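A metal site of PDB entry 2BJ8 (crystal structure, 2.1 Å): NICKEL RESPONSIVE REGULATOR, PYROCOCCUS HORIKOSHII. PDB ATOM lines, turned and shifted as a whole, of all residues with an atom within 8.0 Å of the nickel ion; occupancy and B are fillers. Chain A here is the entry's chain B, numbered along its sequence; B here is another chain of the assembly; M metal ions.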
ATOM      1  N   TYR A  62     -15.705  15.313   6.610  1.00  0.00           N
ATOM      2  CA  TYR A  62     -14.876  16.483   6.403  1.00  0.00           C
ATOM      3  C   TYR A  62     -13.409  16.112   6.294  1.00  0.00           C
ATOM      4  O   TYR A  62     -12.996  15.012   6.642  1.00  0.00           O
ATOM      5  CB  TYR A  62     -15.065  17.472   7.552  1.00  0.00           C
ATOM      6  CG  TYR A  62     -14.734  16.895   8.913  1.00  0.00           C
ATOM      7  CD1 TYR A  62     -13.411  16.826   9.370  1.00  0.00           C
ATOM      8  CD2 TYR A  62     -15.737  16.385   9.739  1.00  0.00           C
ATOM      9  CE1 TYR A  62     -13.110  16.274  10.606  1.00  0.00           C
ATOM     10  CE2 TYR A  62     -15.438  15.824  10.980  1.00  0.00           C
ATOM     11  CZ  TYR A  62     -14.128  15.771  11.415  1.00  0.00           C
ATOM     12  OH  TYR A  62     -13.837  15.214  12.635  1.00  0.00           O
ATOM     13  N   ASN A  63     -12.635  17.056   5.772  1.00  0.00           N
ATOM     14  CA  ASN A  63     -11.195  16.905   5.627  1.00  0.00           C
ATOM     15  C   ASN A  63     -10.635  17.633   6.841  1.00  0.00           C
ATOM     16  O   ASN A  63     -10.750  18.860   6.927  1.00  0.00           O
ATOM     17  CB  ASN A  63     -10.730  17.580   4.338  1.00  0.00           C
ATOM     18  CG  ASN A  63      -9.226  17.511   4.139  1.00  0.00           C
ATOM     19  OD1 ASN A  63      -8.453  17.904   5.011  1.00  0.00           O
ATOM     20  ND2 ASN A  63      -8.808  16.997   2.981  1.00  0.00           N
ATOM     21  N   HIS A  64     -10.054  16.890   7.781  1.00  0.00           N
ATOM     22  CA  HIS A  64      -9.511  17.516   8.990  1.00  0.00           C
ATOM     23  C   HIS A  64      -8.358  18.476   8.747  1.00  0.00           C
ATOM     24  O   HIS A  64      -8.020  19.275   9.619  1.00  0.00           O
ATOM     25  CB  HIS A  64      -9.048  16.454   9.988  1.00  0.00           C
ATOM     26  CG  HIS A  64      -7.891  15.640   9.499  1.00  0.00           C
ATOM     27  ND1 HIS A  64      -8.062  14.511   8.724  1.00  0.00           N
ATOM     28  CD2 HIS A  64      -6.565  15.805   9.643  1.00  0.00           C
ATOM     29  CE1 HIS A  64      -6.876  14.011   8.414  1.00  0.00           C
ATOM     30  NE2 HIS A  64      -5.952  14.784   8.956  1.00  0.00           N
ATOM     31  N   VAL A  70     -11.936  21.370  12.081  1.00  0.00           N
ATOM     32  CA  VAL A  70     -11.754  20.557  13.284  1.00  0.00           C
ATOM     33  C   VAL A  70     -11.973  21.337  14.571  1.00  0.00           C
ATOM     34  O   VAL A  70     -12.693  20.902  15.469  1.00  0.00           O
ATOM     35  CB  VAL A  70     -10.341  19.918  13.323  1.00  0.00           C
ATOM     36  CG1 VAL A  70     -10.129  19.228  14.648  1.00  0.00           C
ATOM     37  CG2 VAL A  70     -10.189  18.913  12.190  1.00  0.00           C
ATOM     38  N   HIS A  89     -15.890   8.487  15.604  1.00  0.00           N
ATOM     39  CA  HIS A  89     -15.085   9.005  14.505  1.00  0.00           C
ATOM     40  C   HIS A  89     -14.361   7.871  13.790  1.00  0.00           C
ATOM     41  O   HIS A  89     -13.815   6.968  14.416  1.00  0.00           O
ATOM     42  CB  HIS A  89     -14.070  10.017  15.044  1.00  0.00           C
ATOM     43  CG  HIS A  89     -13.197  10.632  13.992  1.00  0.00           C
ATOM     44  ND1 HIS A  89     -13.013  11.989  13.878  1.00  0.00           N
ATOM     45  CD2 HIS A  89     -12.413  10.069  13.046  1.00  0.00           C
ATOM     46  CE1 HIS A  89     -12.152  12.235  12.911  1.00  0.00           C
ATOM     47  NE2 HIS A  89     -11.768  11.086  12.394  1.00  0.00           N
ATOM     48  N   VAL A  90     -14.386   7.921  12.462  1.00  0.00           N
ATOM     49  CA  VAL A  90     -13.732   6.927  11.620  1.00  0.00           C
ATOM     50  C   VAL A  90     -12.824   7.656  10.630  1.00  0.00           C
ATOM     51  O   VAL A  90     -13.279   8.558   9.913  1.00  0.00           O
ATOM     52  CB  VAL A  90     -14.754   6.084  10.820  1.00  0.00           C
ATOM     53  CG1 VAL A  90     -14.018   5.108   9.898  1.00  0.00           C
ATOM     54  CG2 VAL A  90     -15.665   5.311  11.767  1.00  0.00           C
ATOM     55  N   HIS A  91     -11.548   7.294  10.595  1.00  0.00           N
ATOM     56  CA  HIS A  91     -10.613   7.923   9.671  1.00  0.00           C
ATOM     57  C   HIS A  91     -10.732   7.200   8.337  1.00  0.00           C
ATOM     58  O   HIS A  91     -10.253   6.070   8.182  1.00  0.00           O
ATOM     59  CB  HIS A  91      -9.186   7.821  10.211  1.00  0.00           C
ATOM     60  CG  HIS A  91      -9.056   8.303  11.621  1.00  0.00           C
ATOM     61  ND1 HIS A  91      -9.477   9.561  12.015  1.00  0.00           N
ATOM     62  CD2 HIS A  91      -8.590   7.704  12.738  1.00  0.00           C
ATOM     63  CE1 HIS A  91      -9.272   9.711  13.311  1.00  0.00           C
ATOM     64  NE2 HIS A  91      -8.736   8.590  13.775  1.00  0.00           N
ATOM     65  N   MET A  92     -11.394   7.857   7.391  1.00  0.00           N
ATOM     66  CA  MET A  92     -11.665   7.320   6.047  1.00  0.00           C
ATOM     67  C   MET A  92     -10.415   7.132   5.203  1.00  0.00           C
ATOM     68  O   MET A  92     -10.187   6.071   4.639  1.00  0.00           O
ATOM     69  CB  MET A  92     -12.622   8.258   5.316  1.00  0.00           C
ATOM     70  CG  MET A  92     -13.973   8.422   6.011  1.00  0.00           C
ATOM     71  SD  MET A  92     -15.071   7.010   5.732  1.00  0.00           S
ATOM     72  CE  MET A  92     -14.441   5.833   6.888  1.00  0.00           C
ATOM     73  N   ASP A  93      -9.609   8.187   5.098  1.00  0.00           N
ATOM     74  CA  ASP A  93      -8.370   8.140   4.345  1.00  0.00           C
ATOM     75  C   ASP A  93      -7.433   9.166   4.962  1.00  0.00           C
ATOM     76  O   ASP A  93      -7.760   9.762   5.988  1.00  0.00           O
ATOM     77  CB  ASP A  93      -8.613   8.453   2.852  1.00  0.00           C
ATOM     78  CG  ASP A  93      -9.312   9.778   2.635  1.00  0.00           C
ATOM     79  OD1 ASP A  93      -8.784  10.822   3.091  1.00  0.00           O
ATOM     80  OD2 ASP A  93     -10.396   9.778   2.010  1.00  0.00           O
ATOM     81  N   GLU A  94      -6.291   9.377   4.326  1.00  0.00           N
ATOM     82  CA  GLU A  94      -5.317  10.315   4.854  1.00  0.00           C
ATOM     83  C   GLU A  94      -5.903  11.666   5.229  1.00  0.00           C
ATOM     84  O   GLU A  94      -5.469  12.288   6.190  1.00  0.00           O
ATOM     85  CB  GLU A  94      -4.191  10.528   3.848  1.00  0.00           C
ATOM     86  CG  GLU A  94      -3.163  11.556   4.289  1.00  0.00           C
ATOM     87  CD  GLU A  94      -2.108  11.827   3.246  1.00  0.00           C
ATOM     88  OE1 GLU A  94      -1.240  12.698   3.495  1.00  0.00           O
ATOM     89  OE2 GLU A  94      -2.144  11.190   2.172  1.00  0.00           O
ATOM     90  N   HIS A  95      -6.916  12.114   4.480  1.00  0.00           N
ATOM     91  CA  HIS A  95      -7.497  13.430   4.743  1.00  0.00           C
ATOM     92  C   HIS A  95      -8.950  13.477   5.223  1.00  0.00           C
ATOM     93  O   HIS A  95      -9.325  14.400   5.934  1.00  0.00           O
ATOM     94  CB  HIS A  95      -7.378  14.296   3.487  1.00  0.00           C
ATOM     95  CG  HIS A  95      -5.955  14.592   3.101  1.00  0.00           C
ATOM     96  ND1 HIS A  95      -5.088  15.262   3.931  1.00  0.00           N
ATOM     97  CD2 HIS A  95      -5.266  14.317   1.967  1.00  0.00           C
ATOM     98  CE1 HIS A  95      -3.914  15.388   3.328  1.00  0.00           C
ATOM     99  NE2 HIS A  95      -4.001  14.823   2.139  1.00  0.00           N
ATOM    100  N   ASN A  96      -9.749  12.491   4.850  1.00  0.00           N
ATOM    101  CA  ASN A  96     -11.155  12.508   5.226  1.00  0.00           C
ATOM    102  C   ASN A  96     -11.561  11.724   6.469  1.00  0.00           C
ATOM    103  O   ASN A  96     -11.137  10.591   6.688  1.00  0.00           O
ATOM    104  CB  ASN A  96     -11.995  12.064   4.035  1.00  0.00           C
ATOM    105  CG  ASN A  96     -11.850  12.994   2.851  1.00  0.00           C
ATOM    106  OD1 ASN A  96     -12.142  14.176   2.937  1.00  0.00           O
ATOM    107  ND2 ASN A  96     -11.386  12.449   1.725  1.00  0.00           N
ATOM    108  N   CYS A  97     -12.401  12.370   7.275  1.00  0.00           N
ATOM    109  CA  CYS A  97     -12.934  11.801   8.508  1.00  0.00           C
ATOM    110  C   CYS A  97     -14.448  11.708   8.428  1.00  0.00           C
ATOM    111  O   CYS A  97     -15.104  12.561   7.825  1.00  0.00           O
ATOM    112  CB  CYS A  97     -12.585  12.702   9.704  1.00  0.00           C
ATOM    113  SG  CYS A  97     -10.826  12.972  10.038  1.00  0.00           S
ATOM    114  N   LEU A  98     -15.000  10.670   9.043  1.00  0.00           N
ATOM    115  CA  LEU A  98     -16.439  10.511   9.099  1.00  0.00           C
ATOM    116  C   LEU A  98     -16.738  10.560  10.587  1.00  0.00           C
ATOM    117  O   LEU A  98     -16.078   9.885  11.383  1.00  0.00           O
ATOM    118  CB  LEU A  98     -16.859   9.159   8.526  1.00  0.00           C
ATOM    119  CG  LEU A  98     -18.382   8.910   8.518  1.00  0.00           C
ATOM    120  CD1 LEU A  98     -18.697   7.736   7.601  1.00  0.00           C
ATOM    121  CD2 LEU A  98     -18.872   8.621   9.920  1.00  0.00           C
ATOM    122  N   GLU A  99     -17.722  11.348  10.982  1.00  0.00           N
ATOM    123  CA  GLU A  99     -18.062  11.460  12.388  1.00  0.00           C
ATOM    124  C   GLU A  99     -19.569  11.426  12.588  1.00  0.00           C
ATOM    125  O   GLU A  99     -20.317  12.070  11.843  1.00  0.00           O
ATOM    126  CB  GLU A  99     -17.495  12.770  12.935  1.00  0.00           C
ATOM    127  CG  GLU A  99     -17.561  12.907  14.448  1.00  0.00           C
ATOM    128  CD  GLU A  99     -16.981  14.220  14.938  1.00  0.00           C
ATOM    129  OE1 GLU A  99     -15.943  14.661  14.382  1.00  0.00           O
ATOM    130  OE2 GLU A  99     -17.552  14.820  15.866  1.00  0.00           O
ATOM    131  N   LEU B  73      -3.062  14.794  17.272  1.00  0.00           N
ATOM    132  CA  LEU B  73      -3.784  13.534  17.470  1.00  0.00           C
ATOM    133  C   LEU B  73      -4.339  12.975  16.159  1.00  0.00           C
ATOM    134  O   LEU B  73      -4.145  11.803  15.860  1.00  0.00           O
ATOM    135  CB  LEU B  73      -4.916  13.710  18.491  1.00  0.00           C
ATOM    136  CG  LEU B  73      -4.480  13.650  19.952  1.00  0.00           C
ATOM    137  CD1 LEU B  73      -5.611  14.126  20.857  1.00  0.00           C
ATOM    138  CD2 LEU B  73      -4.062  12.216  20.302  1.00  0.00           C
ATOM    139  N   LEU B  74      -5.006  13.828  15.392  1.00  0.00           N
ATOM    140  CA  LEU B  74      -5.594  13.420  14.110  1.00  0.00           C
ATOM    141  C   LEU B  74      -4.543  13.009  13.084  1.00  0.00           C
ATOM    142  O   LEU B  74      -4.673  11.963  12.450  1.00  0.00           O
ATOM    143  CB  LEU B  74      -6.436  14.554  13.533  1.00  0.00           C
ATOM    144  CG  LEU B  74      -7.837  14.733  14.095  1.00  0.00           C
ATOM    145  CD1 LEU B  74      -8.468  15.990  13.508  1.00  0.00           C
ATOM    146  CD2 LEU B  74      -8.670  13.505  13.752  1.00  0.00           C
ATOM    147  N   ASP B  75      -3.522  13.840  12.902  1.00  0.00           N
ATOM    148  CA  ASP B  75      -2.471  13.535  11.950  1.00  0.00           C
ATOM    149  C   ASP B  75      -1.815  12.205  12.291  1.00  0.00           C
ATOM    150  O   ASP B  75      -1.569  11.385  11.415  1.00  0.00           O
ATOM    151  CB  ASP B  75      -1.426  14.647  11.949  1.00  0.00           C
ATOM    152  CG  ASP B  75      -1.941  15.931  11.296  1.00  0.00           C
ATOM    153  OD1 ASP B  75      -1.239  16.957  11.398  1.00  0.00           O
ATOM    154  OD2 ASP B  75      -3.026  15.908  10.691  1.00  0.00           O
ATOM    155  N   GLN B  77      -3.119   9.698  14.044  1.00  0.00           N
ATOM    156  CA  GLN B  77      -4.079   8.613  13.826  1.00  0.00           C
ATOM    157  C   GLN B  77      -4.281   8.313  12.348  1.00  0.00           C
ATOM    158  O   GLN B  77      -4.385   7.152  11.957  1.00  0.00           O
ATOM    159  CB  GLN B  77      -5.427   8.947  14.473  1.00  0.00           C
ATOM    160  CG  GLN B  77      -5.397   8.880  15.998  1.00  0.00           C
ATOM    161  CD  GLN B  77      -6.754   9.139  16.627  1.00  0.00           C
ATOM    162  OE1 GLN B  77      -7.727   8.407  16.393  1.00  0.00           O
ATOM    163  NE2 GLN B  77      -6.834  10.190  17.433  1.00  0.00           N
ATOM    164  N   HIS B  78      -4.325   9.363  11.528  1.00  0.00           N
ATOM    165  CA  HIS B  78      -4.521   9.154  10.099  1.00  0.00           C
ATOM    166  C   HIS B  78      -3.305   8.520   9.404  1.00  0.00           C
ATOM    167  O   HIS B  78      -3.389   8.137   8.236  1.00  0.00           O
ATOM    168  CB  HIS B  78      -4.908  10.467   9.432  1.00  0.00           C
ATOM    169  CG  HIS B  78      -6.368  10.770   9.525  1.00  0.00           C
ATOM    170  ND1 HIS B  78      -7.223  10.663   8.445  1.00  0.00           N
ATOM    171  CD2 HIS B  78      -7.149  11.122  10.579  1.00  0.00           C
ATOM    172  CE1 HIS B  78      -8.450  10.937   8.833  1.00  0.00           C
ATOM    173  NE2 HIS B  78      -8.433  11.217  10.126  1.00  0.00           N
ATOM    174  N   LEU B  81      -4.026   4.221   9.451  1.00  0.00           N
ATOM    175  CA  LEU B  81      -5.380   3.841   9.070  1.00  0.00           C
ATOM    176  C   LEU B  81      -5.628   2.347   9.220  1.00  0.00           C
ATOM    177  O   LEU B  81      -6.730   1.926   9.553  1.00  0.00           O
ATOM    178  CB  LEU B  81      -5.660   4.257   7.623  1.00  0.00           C
ATOM    179  CG  LEU B  81      -5.581   5.737   7.263  1.00  0.00           C
ATOM    180  CD1 LEU B  81      -5.839   5.919   5.775  1.00  0.00           C
ATOM    181  CD2 LEU B  81      -6.590   6.523   8.074  1.00  0.00           C
ATOM    182  N   ILE B  84      -5.912   1.614  13.364  1.00  0.00           N
ATOM    183  CA  ILE B  84      -6.974   2.313  14.066  1.00  0.00           C
ATOM    184  C   ILE B  84      -8.336   2.079  13.420  1.00  0.00           C
ATOM    185  O   ILE B  84      -8.577   2.485  12.295  1.00  0.00           O
ATOM    186  CB  ILE B  84      -6.681   3.826  14.137  1.00  0.00           C
ATOM    187  CG1 ILE B  84      -5.404   4.061  14.943  1.00  0.00           C
ATOM    188  CG2 ILE B  84      -7.850   4.565  14.768  1.00  0.00           C
ATOM    189  CD1 ILE B  84      -4.990   5.507  15.037  1.00  0.00           C
ATOM    190  N   SER B  87     -12.809   5.687  16.890  1.00  0.00           N
ATOM    191  CA  SER B  87     -12.573   6.328  18.170  1.00  0.00           C
ATOM    192  C   SER B  87     -13.874   6.929  18.709  1.00  0.00           C
ATOM    193  O   SER B  87     -14.711   7.412  17.940  1.00  0.00           O
ATOM    194  CB  SER B  87     -11.510   7.419  18.069  1.00  0.00           C
ATOM    195  OG  SER B  87     -11.955   8.492  17.263  1.00  0.00           O
HETATM  196 NI    NI M   1     -10.158  11.147  11.187  1.00  0.00          NI
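N of Cys 97 is in hydrogen-bond range of O of Tyr 62, 2.8 Å away. O of Ser 87 of chain B sits at hydrogen-bond distance from N of His 89 (2.8 Å). The side-chain sulfur (SG) of Cys 97 sits close to a ring nitrogen (ND1) of His 64, 3.4 Å away. A ring nitrogen (ND1) of His 78 of chain B sits at hydrogen-bond distance from the backbone carbonyl oxygen (O) of Asp 93. A ring nitrogen (NE2) of His 91 sits at hydrogen-bond distance from the side-chain amide oxygen of Gln 77 of chain B (2.8 Å). A ring nitrogen (ND1) of His 78 of chain B sits at hydrogen-bond distance from the backbone carbonyl oxygen of Glu 94 (3.3 Å).
The nickel ion is bound by a ring nitrogen (ND1) of His 91 (1.9 Å), a ring nitrogen (NE2) of His 89 (2.0 Å), a ring nitrogen (NE2) of His 78 of chain B (2.0 Å) and the side-chain sulfur (SG) of Cys 97 (2.3 Å). The nickel ion has four donor atoms within binding distance.
Merely in contact with the nickel ion: Leu 74 of chain B (3.8 Å). Of the 23 residues printed, 5 come within 4 Å of the nickel ion. The nearest printed residue that does not touch the nickel ion is Val 90 (4.3 Å).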
